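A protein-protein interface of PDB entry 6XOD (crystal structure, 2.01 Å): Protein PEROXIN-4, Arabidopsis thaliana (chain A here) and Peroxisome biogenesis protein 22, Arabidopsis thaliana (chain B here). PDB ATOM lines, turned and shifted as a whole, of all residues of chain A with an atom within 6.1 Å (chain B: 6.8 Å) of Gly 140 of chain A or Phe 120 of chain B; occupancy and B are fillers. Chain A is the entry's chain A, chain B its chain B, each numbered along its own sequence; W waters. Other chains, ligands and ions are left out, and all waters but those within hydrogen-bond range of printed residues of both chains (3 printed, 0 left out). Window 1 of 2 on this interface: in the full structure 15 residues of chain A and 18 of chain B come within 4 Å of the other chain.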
ATOM      1  N   PHE A  79       8.552 -26.274 -10.555  1.00  0.00           N
ATOM      2  CA  PHE A  79       8.576 -26.652 -11.964  1.00  0.00           C
ATOM      3  C   PHE A  79       9.297 -27.993 -12.051  1.00  0.00           C
ATOM      4  O   PHE A  79      10.525 -28.060 -11.945  1.00  0.00           O
ATOM      5  CB  PHE A  79       9.264 -25.566 -12.784  1.00  0.00           C
ATOM      6  CG  PHE A  79       9.313 -25.844 -14.253  1.00  0.00           C
ATOM      7  CD1 PHE A  79       8.228 -25.553 -15.062  1.00  0.00           C
ATOM      8  CD2 PHE A  79      10.456 -26.370 -14.832  1.00  0.00           C
ATOM      9  CE1 PHE A  79       8.274 -25.799 -16.415  1.00  0.00           C
ATOM     10  CE2 PHE A  79      10.509 -26.615 -16.186  1.00  0.00           C
ATOM     11  CZ  PHE A  79       9.417 -26.328 -16.980  1.00  0.00           C
ATOM     12  N   ASP A 128       5.360 -29.614 -20.114  1.00  0.00           N
ATOM     13  CA  ASP A 128       6.377 -28.679 -20.583  1.00  0.00           C
ATOM     14  C   ASP A 128       7.704 -28.921 -19.877  1.00  0.00           C
ATOM     15  O   ASP A 128       8.767 -28.886 -20.507  1.00  0.00           O
ATOM     16  CB  ASP A 128       5.907 -27.242 -20.368  1.00  0.00           C
ATOM     17  CG  ASP A 128       4.639 -26.921 -21.138  1.00  0.00           C
ATOM     18  OD1 ASP A 128       4.545 -27.314 -22.320  1.00  0.00           O
ATOM     19  OD2 ASP A 128       3.733 -26.286 -20.558  1.00  0.00           O
ATOM     20  N   LEU A 132      11.114 -30.584 -21.964  1.00  0.00           N
ATOM     21  CA  LEU A 132      12.468 -30.039 -21.967  1.00  0.00           C
ATOM     22  C   LEU A 132      13.498 -31.129 -21.693  1.00  0.00           C
ATOM     23  O   LEU A 132      14.553 -31.173 -22.338  1.00  0.00           O
ATOM     24  CB  LEU A 132      12.578 -28.915 -20.936  1.00  0.00           C
ATOM     25  CG  LEU A 132      11.905 -27.595 -21.325  1.00  0.00           C
ATOM     26  CD1 LEU A 132      11.683 -26.726 -20.102  1.00  0.00           C
ATOM     27  CD2 LEU A 132      12.741 -26.847 -22.354  1.00  0.00           C
ATOM     28  N   ASP A 137      16.939 -30.882 -23.661  1.00  0.00           N
ATOM     29  CA  ASP A 137      17.206 -29.484 -23.323  1.00  0.00           C
ATOM     30  C   ASP A 137      17.358 -29.349 -21.807  1.00  0.00           C
ATOM     31  O   ASP A 137      16.520 -28.785 -21.102  1.00  0.00           O
ATOM     32  CB  ASP A 137      16.097 -28.587 -23.859  1.00  0.00           C
ATOM     33  CG  ASP A 137      16.508 -27.132 -23.928  1.00  0.00           C
ATOM     34  OD1 ASP A 137      17.338 -26.704 -23.097  1.00  0.00           O
ATOM     35  OD2 ASP A 137      16.002 -26.417 -24.817  1.00  0.00           O
ATOM     36  N   VAL A 138      18.473 -29.886 -21.311  1.00  0.00           N
ATOM     37  CA  VAL A 138      18.724 -29.876 -19.874  1.00  0.00           C
ATOM     38  C   VAL A 138      18.983 -28.457 -19.385  1.00  0.00           C
ATOM     39  O   VAL A 138      18.538 -28.073 -18.296  1.00  0.00           O
ATOM     40  CB  VAL A 138      19.894 -30.818 -19.534  1.00  0.00           C
ATOM     41  CG1 VAL A 138      20.202 -30.778 -18.044  1.00  0.00           C
ATOM     42  CG2 VAL A 138      19.570 -32.236 -19.976  1.00  0.00           C
ATOM     43  N   ARG A 139      19.705 -27.657 -20.172  1.00  0.00           N
ATOM     44  CA  ARG A 139      19.918 -26.263 -19.795  1.00  0.00           C
ATOM     45  C   ARG A 139      18.592 -25.535 -19.636  1.00  0.00           C
ATOM     46  O   ARG A 139      18.403 -24.771 -18.682  1.00  0.00           O
ATOM     47  CB  ARG A 139      20.792 -25.559 -20.833  1.00  0.00           C
ATOM     48  CG  ARG A 139      21.100 -24.105 -20.495  1.00  0.00           C
ATOM     49  CD  ARG A 139      21.929 -23.436 -21.582  1.00  0.00           C
ATOM     50  NE  ARG A 139      23.213 -24.100 -21.787  1.00  0.00           N
ATOM     51  CZ  ARG A 139      24.291 -23.900 -21.033  1.00  0.00           C
ATOM     52  NH1 ARG A 139      24.248 -23.060 -20.007  1.00  0.00           N
ATOM     53  NH2 ARG A 139      25.414 -24.550 -21.302  1.00  0.00           N
ATOM     54  N   GLY A 140      17.659 -25.760 -20.564  1.00  0.00           N
ATOM     55  CA  GLY A 140      16.358 -25.123 -20.458  1.00  0.00           C
ATOM     56  C   GLY A 140      15.591 -25.573 -19.230  1.00  0.00           C
ATOM     57  O   GLY A 140      14.991 -24.755 -18.527  1.00  0.00           O
ATOM     58  N   PHE A 141      15.593 -26.879 -18.958  1.00  0.00           N
ATOM     59  CA  PHE A 141      14.932 -27.378 -17.759  1.00  0.00           C
ATOM     60  C   PHE A 141      15.521 -26.736 -16.509  1.00  0.00           C
ATOM     61  O   PHE A 141      14.788 -26.226 -15.652  1.00  0.00           O
ATOM     62  CB  PHE A 141      15.049 -28.899 -17.676  1.00  0.00           C
ATOM     63  CG  PHE A 141      14.619 -29.455 -16.349  1.00  0.00           C
ATOM     64  CD1 PHE A 141      13.278 -29.651 -16.069  1.00  0.00           C
ATOM     65  CD2 PHE A 141      15.555 -29.762 -15.375  1.00  0.00           C
ATOM     66  CE1 PHE A 141      12.879 -30.149 -14.845  1.00  0.00           C
ATOM     67  CE2 PHE A 141      15.159 -30.262 -14.149  1.00  0.00           C
ATOM     68  CZ  PHE A 141      13.819 -30.454 -13.886  1.00  0.00           C
ATOM     69  N   ASN A 142      16.849 -26.762 -16.383  1.00  0.00           N
ATOM     70  CA  ASN A 142      17.486 -26.163 -15.215  1.00  0.00           C
ATOM     71  C   ASN A 142      17.198 -24.671 -15.137  1.00  0.00           C
ATOM     72  O   ASN A 142      16.977 -24.129 -14.047  1.00  0.00           O
ATOM     73  CB  ASN A 142      18.995 -26.410 -15.252  1.00  0.00           C
ATOM     74  CG  ASN A 142      19.356 -27.866 -15.035  1.00  0.00           C
ATOM     75  OD1 ASN A 142      18.545 -28.651 -14.544  1.00  0.00           O
ATOM     76  ND2 ASN A 142      20.581 -28.233 -15.394  1.00  0.00           N
ATOM     77  N   SER A 143      17.193 -23.989 -16.285  1.00  0.00           N
ATOM     78  CA  SER A 143      16.969 -22.547 -16.292  1.00  0.00           C
ATOM     79  C   SER A 143      15.589 -22.205 -15.741  1.00  0.00           C
ATOM     80  O   SER A 143      15.456 -21.349 -14.858  1.00  0.00           O
ATOM     81  CB  SER A 143      17.144 -22.003 -17.713  1.00  0.00           C
ATOM     82  OG  SER A 143      16.879 -20.611 -17.772  1.00  0.00           O
ATOM     83  N   MET A 144      14.547 -22.878 -16.237  1.00  0.00           N
ATOM     84  CA  MET A 144      13.195 -22.564 -15.786  1.00  0.00           C
ATOM     85  C   MET A 144      12.941 -23.098 -14.381  1.00  0.00           C
ATOM     86  O   MET A 144      12.258 -22.450 -13.579  1.00  0.00           O
ATOM     87  CB  MET A 144      12.167 -23.124 -16.771  1.00  0.00           C
ATOM     88  CG  MET A 144      10.721 -22.943 -16.319  1.00  0.00           C
ATOM     89  SD  MET A 144       9.536 -22.824 -17.673  1.00  0.00           S
ATOM     90  CE  MET A 144       9.661 -21.081 -18.072  1.00  0.00           C
ATOM     91  N   ALA A 145      13.483 -24.273 -14.056  1.00  0.00           N
ATOM     92  CA  ALA A 145      13.317 -24.793 -12.703  1.00  0.00           C
ATOM     93  C   ALA A 145      14.012 -23.895 -11.689  1.00  0.00           C
ATOM     94  O   ALA A 145      13.506 -23.686 -10.581  1.00  0.00           O
ATOM     95  CB  ALA A 145      13.854 -26.221 -12.612  1.00  0.00           C
ATOM     96  N   THR B  34       6.457 -12.827 -23.263  1.00  0.00           N
ATOM     97  CA  THR B  34       7.698 -13.560 -23.466  1.00  0.00           C
ATOM     98  C   THR B  34       8.315 -13.108 -24.783  1.00  0.00           C
ATOM     99  O   THR B  34       7.603 -12.720 -25.714  1.00  0.00           O
ATOM    100  CB  THR B  34       7.469 -15.080 -23.485  1.00  0.00           C
ATOM    101  OG1 THR B  34       6.516 -15.419 -24.500  1.00  0.00           O
ATOM    102  CG2 THR B  34       6.967 -15.566 -22.133  1.00  0.00           C
ATOM    103  N   LEU B  75      12.485 -12.797 -20.813  1.00  0.00           N
ATOM    104  CA  LEU B  75      13.380 -12.935 -21.950  1.00  0.00           C
ATOM    105  C   LEU B  75      13.993 -14.331 -21.954  1.00  0.00           C
ATOM    106  O   LEU B  75      14.242 -14.923 -20.903  1.00  0.00           O
ATOM    107  CB  LEU B  75      14.478 -11.872 -21.901  1.00  0.00           C
ATOM    108  CG  LEU B  75      13.985 -10.422 -21.872  1.00  0.00           C
ATOM    109  CD1 LEU B  75      15.152  -9.448 -21.883  1.00  0.00           C
ATOM    110  CD2 LEU B  75      13.051 -10.143 -23.044  1.00  0.00           C
ATOM    111  N   MET B  76      14.234 -14.854 -23.154  1.00  0.00           N
ATOM    112  CA  MET B  76      14.689 -16.229 -23.296  1.00  0.00           C
ATOM    113  C   MET B  76      15.518 -16.357 -24.563  1.00  0.00           C
ATOM    114  O   MET B  76      15.279 -15.655 -25.548  1.00  0.00           O
ATOM    115  CB  MET B  76      13.500 -17.194 -23.335  1.00  0.00           C
ATOM    116  CG  MET B  76      12.457 -16.831 -24.380  1.00  0.00           C
ATOM    117  SD  MET B  76      10.985 -17.863 -24.300  1.00  0.00           S
ATOM    118  CE  MET B  76      10.294 -17.359 -22.723  1.00  0.00           C
ATOM    119  N   GLU B  77      16.501 -17.254 -24.532  1.00  0.00           N
ATOM    120  CA  GLU B  77      17.310 -17.448 -25.724  1.00  0.00           C
ATOM    121  C   GLU B  77      18.055 -18.771 -25.664  1.00  0.00           C
ATOM    122  O   GLU B  77      18.409 -19.261 -24.588  1.00  0.00           O
ATOM    123  CB  GLU B  77      18.307 -16.301 -25.913  1.00  0.00           C
ATOM    124  CG  GLU B  77      18.961 -16.302 -27.282  1.00  0.00           C
ATOM    125  CD  GLU B  77      17.941 -16.337 -28.402  1.00  0.00           C
ATOM    126  OE1 GLU B  77      17.344 -15.279 -28.695  1.00  0.00           O
ATOM    127  OE2 GLU B  77      17.719 -17.429 -28.967  1.00  0.00           O
ATOM    128  N   LEU B 109      15.705 -16.339 -19.257  1.00  0.00           N
ATOM    129  CA  LEU B 109      15.813 -17.786 -19.351  1.00  0.00           C
ATOM    130  C   LEU B 109      16.745 -18.181 -20.488  1.00  0.00           C
ATOM    131  O   LEU B 109      16.959 -17.429 -21.443  1.00  0.00           O
ATOM    132  CB  LEU B 109      14.431 -18.416 -19.558  1.00  0.00           C
ATOM    133  CG  LEU B 109      13.451 -18.240 -18.397  1.00  0.00           C
ATOM    134  CD1 LEU B 109      12.010 -18.238 -18.902  1.00  0.00           C
ATOM    135  CD2 LEU B 109      13.650 -19.334 -17.357  1.00  0.00           C
ATOM    136  N   PHE B 110      17.299 -19.385 -20.375  1.00  0.00           N
ATOM    137  CA  PHE B 110      18.258 -19.897 -21.340  1.00  0.00           C
ATOM    138  C   PHE B 110      17.974 -21.365 -21.608  1.00  0.00           C
ATOM    139  O   PHE B 110      17.581 -22.104 -20.702  1.00  0.00           O
ATOM    140  CB  PHE B 110      19.696 -19.728 -20.839  1.00  0.00           C
ATOM    141  CG  PHE B 110      20.103 -18.298 -20.643  1.00  0.00           C
ATOM    142  CD1 PHE B 110      20.434 -17.506 -21.729  1.00  0.00           C
ATOM    143  CD2 PHE B 110      20.156 -17.745 -19.375  1.00  0.00           C
ATOM    144  CE1 PHE B 110      20.809 -16.189 -21.556  1.00  0.00           C
ATOM    145  CE2 PHE B 110      20.531 -16.427 -19.194  1.00  0.00           C
ATOM    146  CZ  PHE B 110      20.858 -15.648 -20.289  1.00  0.00           C
ATOM    147  N   CYS B 111      18.182 -21.781 -22.855  1.00  0.00           N
ATOM    148  CA  CYS B 111      17.951 -23.161 -23.254  1.00  0.00           C
ATOM    149  C   CYS B 111      18.991 -23.543 -24.301  1.00  0.00           C
ATOM    150  O   CYS B 111      19.822 -22.727 -24.710  1.00  0.00           O
ATOM    151  CB  CYS B 111      16.520 -23.350 -23.772  1.00  0.00           C
ATOM    152  SG  CYS B 111      16.040 -22.266 -25.140  1.00  0.00           S
ATOM    153  N   SER B 112      18.949 -24.806 -24.721  1.00  0.00           N
ATOM    154  CA  SER B 112      19.877 -25.324 -25.716  1.00  0.00           C
ATOM    155  C   SER B 112      19.199 -25.711 -27.023  1.00  0.00           C
ATOM    156  O   SER B 112      19.891 -26.099 -27.968  1.00  0.00           O
ATOM    157  CB  SER B 112      20.631 -26.535 -25.151  1.00  0.00           C
ATOM    158  OG  SER B 112      19.733 -27.531 -24.698  1.00  0.00           O
ATOM    159  N   THR B 113      17.874 -25.607 -27.113  1.00  0.00           N
ATOM    160  CA  THR B 113      17.149 -25.970 -28.321  1.00  0.00           C
ATOM    161  C   THR B 113      16.141 -24.883 -28.666  1.00  0.00           C
ATOM    162  O   THR B 113      15.619 -24.193 -27.787  1.00  0.00           O
ATOM    163  CB  THR B 113      16.415 -27.311 -28.165  1.00  0.00           C
ATOM    164  OG1 THR B 113      15.334 -27.163 -27.236  1.00  0.00           O
ATOM    165  CG2 THR B 113      17.368 -28.387 -27.666  1.00  0.00           C
ATOM    166  N   ILE B 115      13.095 -25.406 -29.942  1.00  0.00           N
ATOM    167  CA  ILE B 115      11.783 -25.814 -29.458  1.00  0.00           C
ATOM    168  C   ILE B 115      11.691 -25.722 -27.941  1.00  0.00           C
ATOM    169  O   ILE B 115      10.584 -25.712 -27.391  1.00  0.00           O
ATOM    170  CB  ILE B 115      11.469 -27.233 -29.971  1.00  0.00           C
ATOM    171  CG1 ILE B 115      11.283 -27.200 -31.492  1.00  0.00           C
ATOM    172  CG2 ILE B 115      10.225 -27.790 -29.302  1.00  0.00           C
ATOM    173  CD1 ILE B 115      11.391 -28.551 -32.163  1.00  0.00           C
ATOM    174  N   GLY B 116      12.824 -25.641 -27.244  1.00  0.00           N
ATOM    175  CA  GLY B 116      12.778 -25.407 -25.812  1.00  0.00           C
ATOM    176  C   GLY B 116      12.066 -24.118 -25.455  1.00  0.00           C
ATOM    177  O   GLY B 116      11.431 -24.026 -24.401  1.00  0.00           O
ATOM    178  N   ARG B 117      12.153 -23.108 -26.326  1.00  0.00           N
ATOM    179  CA  ARG B 117      11.444 -21.859 -26.073  1.00  0.00           C
ATOM    180  C   ARG B 117       9.940 -22.084 -26.027  1.00  0.00           C
ATOM    181  O   ARG B 117       9.234 -21.446 -25.239  1.00  0.00           O
ATOM    182  CB  ARG B 117      11.791 -20.820 -27.140  1.00  0.00           C
ATOM    183  CG  ARG B 117      13.164 -20.197 -26.968  1.00  0.00           C
ATOM    184  CD  ARG B 117      13.238 -18.813 -27.598  1.00  0.00           C
ATOM    185  NE  ARG B 117      13.020 -18.832 -29.042  1.00  0.00           N
ATOM    186  CZ  ARG B 117      13.926 -19.225 -29.934  1.00  0.00           C
ATOM    187  NH1 ARG B 117      15.118 -19.651 -29.533  1.00  0.00           N
ATOM    188  NH2 ARG B 117      13.640 -19.199 -31.226  1.00  0.00           N
ATOM    189  N   THR B 118       9.428 -22.986 -26.867  1.00  0.00           N
ATOM    190  CA  THR B 118       7.998 -23.266 -26.839  1.00  0.00           C
ATOM    191  C   THR B 118       7.579 -23.843 -25.494  1.00  0.00           C
ATOM    192  O   THR B 118       6.454 -23.604 -25.038  1.00  0.00           O
ATOM    193  CB  THR B 118       7.619 -24.223 -27.970  1.00  0.00           C
ATOM    194  OG1 THR B 118       8.156 -25.526 -27.709  1.00  0.00           O
ATOM    195  CG2 THR B 118       8.153 -23.714 -29.301  1.00  0.00           C
ATOM    196  N   SER B 119       8.467 -24.597 -24.842  1.00  0.00           N
ATOM    197  CA  SER B 119       8.158 -25.114 -23.513  1.00  0.00           C
ATOM    198  C   SER B 119       8.114 -23.992 -22.481  1.00  0.00           C
ATOM    199  O   SER B 119       7.222 -23.966 -21.625  1.00  0.00           O
ATOM    200  CB  SER B 119       9.180 -26.177 -23.115  1.00  0.00           C
ATOM    201  OG  SER B 119       9.065 -27.322 -23.942  1.00  0.00           O
ATOM    202  N   PHE B 120       9.072 -23.063 -22.538  1.00  0.00           N
ATOM    203  CA  PHE B 120       9.015 -21.885 -21.678  1.00  0.00           C
ATOM    204  C   PHE B 120       7.680 -21.165 -21.828  1.00  0.00           C
ATOM    205  O   PHE B 120       7.002 -20.868 -20.839  1.00  0.00           O
ATOM    206  CB  PHE B 120      10.155 -20.920 -22.015  1.00  0.00           C
ATOM    207  CG  PHE B 120      11.529 -21.419 -21.649  1.00  0.00           C
ATOM    208  CD1 PHE B 120      11.708 -22.492 -20.790  1.00  0.00           C
ATOM    209  CD2 PHE B 120      12.650 -20.787 -22.159  1.00  0.00           C
ATOM    210  CE1 PHE B 120      12.978 -22.929 -20.459  1.00  0.00           C
ATOM    211  CE2 PHE B 120      13.921 -21.221 -21.834  1.00  0.00           C
ATOM    212  CZ  PHE B 120      14.084 -22.291 -20.984  1.00  0.00           C
ATOM    213  N   VAL B 121       7.295 -20.870 -23.071  1.00  0.00           N
ATOM    214  CA  VAL B 121       6.132 -20.020 -23.314  1.00  0.00           C
ATOM    215  C   VAL B 121       4.851 -20.718 -22.878  1.00  0.00           C
ATOM    216  O   VAL B 121       3.981 -20.104 -22.247  1.00  0.00           O
ATOM    217  CB  VAL B 121       6.076 -19.616 -24.800  1.00  0.00           C
ATOM    218  CG1 VAL B 121       4.804 -18.839 -25.096  1.00  0.00           C
ATOM    219  CG2 VAL B 121       7.302 -18.796 -25.176  1.00  0.00           C
ATOM    220  N   ARG B 122       4.703 -22.002 -23.213  1.00  0.00           N
ATOM    221  CA  ARG B 122       3.481 -22.714 -22.851  1.00  0.00           C
ATOM    222  C   ARG B 122       3.334 -22.837 -21.342  1.00  0.00           C
ATOM    223  O   ARG B 122       2.210 -22.870 -20.827  1.00  0.00           O
ATOM    224  CB  ARG B 122       3.468 -24.097 -23.502  1.00  0.00           C
ATOM    225  CG  ARG B 122       3.169 -24.076 -24.997  1.00  0.00           C
ATOM    226  CD  ARG B 122       3.266 -25.463 -25.633  1.00  0.00           C
ATOM    227  NE  ARG B 122       2.901 -26.540 -24.718  1.00  0.00           N
ATOM    228  CZ  ARG B 122       2.793 -27.818 -25.067  1.00  0.00           C
ATOM    229  NH1 ARG B 122       3.015 -28.192 -26.321  1.00  0.00           N
ATOM    230  NH2 ARG B 122       2.459 -28.723 -24.157  1.00  0.00           N
ATOM    231  N   GLN B 123       4.451 -22.915 -20.618  1.00  0.00           N
ATOM    232  CA  GLN B 123       4.391 -22.908 -19.160  1.00  0.00           C
ATOM    233  C   GLN B 123       3.993 -21.533 -18.641  1.00  0.00           C
ATOM    234  O   GLN B 123       3.179 -21.425 -17.719  1.00  0.00           O
ATOM    235  CB  GLN B 123       5.745 -23.337 -18.589  1.00  0.00           C
ATOM    236  CG  GLN B 123       5.970 -23.020 -17.112  1.00  0.00           C
ATOM    237  CD  GLN B 123       5.125 -23.867 -16.181  1.00  0.00           C
ATOM    238  OE1 GLN B 123       4.800 -25.016 -16.484  1.00  0.00           O
ATOM    239  NE2 GLN B 123       4.768 -23.303 -15.034  1.00  0.00           N
ATOM    240  N   LEU B 124       4.551 -20.472 -19.227  1.00  0.00           N
ATOM    241  CA  LEU B 124       4.324 -19.123 -18.727  1.00  0.00           C
ATOM    242  C   LEU B 124       2.987 -18.547 -19.166  1.00  0.00           C
ATOM    243  O   LEU B 124       2.466 -17.650 -18.492  1.00  0.00           O
ATOM    244  CB  LEU B 124       5.465 -18.207 -19.179  1.00  0.00           C
ATOM    245  CG  LEU B 124       6.775 -18.406 -18.409  1.00  0.00           C
ATOM    246  CD1 LEU B 124       7.950 -17.765 -19.131  1.00  0.00           C
ATOM    247  CD2 LEU B 124       6.636 -17.842 -16.999  1.00  0.00           C
ATOM    248  N   GLU B 125       2.420 -19.040 -20.264  1.00  0.00           N
ATOM    249  CA  GLU B 125       1.112 -18.616 -20.743  1.00  0.00           C
ATOM    250  C   GLU B 125       1.009 -17.092 -20.834  1.00  0.00           C
ATOM    251  O   GLU B 125       0.103 -16.486 -20.252  1.00  0.00           O
ATOM    252  CB  GLU B 125       0.008 -19.177 -19.852  1.00  0.00           C
ATOM    253  CG  GLU B 125      -0.026 -20.692 -19.809  1.00  0.00           C
ATOM    254  CD  GLU B 125      -1.243 -21.221 -19.082  1.00  0.00           C
ATOM    255  OE1 GLU B 125      -2.085 -20.400 -18.659  1.00  0.00           O
ATOM    256  OE2 GLU B 125      -1.360 -22.455 -18.926  1.00  0.00           O
ATOM    257  N   PRO B 126       1.916 -16.444 -21.557  1.00  0.00           N
ATOM    258  CA  PRO B 126       1.826 -14.991 -21.720  1.00  0.00           C
ATOM    259  C   PRO B 126       0.688 -14.615 -22.656  1.00  0.00           C
ATOM    260  O   PRO B 126       0.106 -15.446 -23.356  1.00  0.00           O
ATOM    261  CB  PRO B 126       3.185 -14.616 -22.313  1.00  0.00           C
ATOM    262  CG  PRO B 126       3.587 -15.836 -23.074  1.00  0.00           C
ATOM    263  CD  PRO B 126       3.084 -17.002 -22.265  1.00  0.00           C
HETATM  264  O   HOH W   1       6.463 -28.305 -24.249  1.00  0.00           O
HETATM  265  O   HOH W   2      21.193 -28.771 -22.707  1.00  0.00           O
HETATM  266  O   HOH W   3       3.087 -26.293 -17.960  1.00  0.00           O
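OD1 of Asp 128 of chain A is in salt-bridge range of NE of Arg 122 of chain B, at 3.0 Å.
OD2 of Asp 128 of chain A sits at hydrogen-bond distance from N of Gln 123 of chain B (3.4 Å).
The backbone NH (N) of Ser 112 of chain B is in hydrogen-bond range of the side-chain carboxylate (OD1) of Asp 137 of chain A (3.0 Å).
The side-chain carboxylate (OD2) of Asp 137 of chain A is in hydrogen-bond range of the side-chain hydroxyl (OG1) of Thr 113 of chain B.
The side-chain hydroxyl (OG) of Ser 143 of chain A lies within hydrogen-bond range of the backbone NH (N) of Phe 110 of chain B (2.9 Å).
The backbone carbonyl oxygen (O) of Arg 139 of chain A lies close to the backbone carbonyl oxygen (O) of Phe 110 of chain B, 3.4 Å away.
Gly 140 of chain A touches just these residues of chain B: Phe 110, Cys 111 and Phe 120.
Phe 120 of chain B touches just these residues of chain A: Gly 140 (3.3 Å) and Met 144 (3.7 Å).
Printed residues of chain A within 4 Å of Ser 112 of chain B: Asp 137.
Printed residues of chain A within 4 Å of Gly 116 of chain B: Leu 132 (3.7 Å) and Asp 137 (3.5 Å).
Ala 145 of chain A touches none of the printed residues of chain B.
Phe 141 of chain A touches none of the printed residues of chain B.
Of the 21 printed residues of chain B, 11 touch a printed residue of chain A.
Printed residues of chain B that touch a printed residue of chain A: Leu 109, Phe 110, Cys 111, Ser 112, Thr 113, Gly 116, Ser 119, Phe 120, Arg 122, Gln 123 and Leu 124.
Hydrophobic or aromatic side chains of chain B that line the printed part of chain A: Leu 109, Phe 120 and Leu 124.
Hydrophobic or aromatic side chains of chain A that line the printed part of chain B: Phe 79, Leu 132 and Met 144.
Among the printed residues, 21 pairs touch across the chains.
Among the printed residues, Asp or Glu carboxylates within 4 Å of a Lys or Arg side-chain nitrogen of the other chain: Asp 128 of chain A with Arg 122 of chain B.
The backbone NH (N) of Asp 137 of chain A is in hydrogen-bond range of the backbone carbonyl oxygen (O) of Leu 132 of chain A, at 2.7 Å.
The backbone NH (N) of Gly 140 of chain A sits at hydrogen-bond distance from the side-chain carboxylate (OD1) of Asp 137 of chain A (2.7 Å).
O of Leu 75 of chain B sits at hydrogen-bond distance from N of Leu 109 of chain B, 2.6 Å away.
The backbone NH of Glu 77 of chain B sits at hydrogen-bond distance from the backbone carbonyl oxygen of Leu 109 of chain B (3.1 Å).
The backbone NH of Cys 111 of chain B is in hydrogen-bond range of the backbone carbonyl oxygen of Glu 77 of chain B.
The side-chain hydroxyl of Thr 113 of chain B is in hydrogen-bond range of the backbone NH of Gly 116 of chain B (2.9 Å).
Water W3 bridges the side-chain amide oxygen (OE1) of Gln 123 of chain B (2.6 Å) and the side-chain carboxylate (OD2) of Asp 128 of chain A (2.7 Å).
Water W2 lies within hydrogen-bond range of the side-chain hydroxyl of Ser 112 of chain B (2.8 Å), the backbone NH of Arg 139 of chain A (3.1 Å) and the backbone NH of Val 138 of chain A (3.3 Å).
Water W1 bridges OG of Ser 119 of chain B (2.8 Å) and OD1 of Asp 128 of chain A (2.9 Å).
Among the printed residues, merely in contact across the chains: Phe 79 of chain A with Gln 123 of chain B, Asp 128 of chain A with Ser 119 of chain B, Leu 132 of chain A with Gly 116 of chain B, Leu 132 of chain A with Ser 119 of chain B, Asp 137 of chain A with Cys 111 of chain B, Asp 137 of chain A with Gly 116 of chain B, Arg 139 of chain A with Cys 111 of chain B, Gly 140 of chain A with Phe 110 of chain B, Gly 140 of chain A with Cys 111 of chain B, Gly 140 of chain A with Phe 120 of chain B, Ser 143 of chain A with Leu 109 of chain B, Met 144 of chain A with Leu 109 of chain B, Met 144 of chain A with Phe 120 of chain B, Met 144 of chain A with Gln 123 of chain B and Met 144 of chain A with Leu 124 of chain B.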
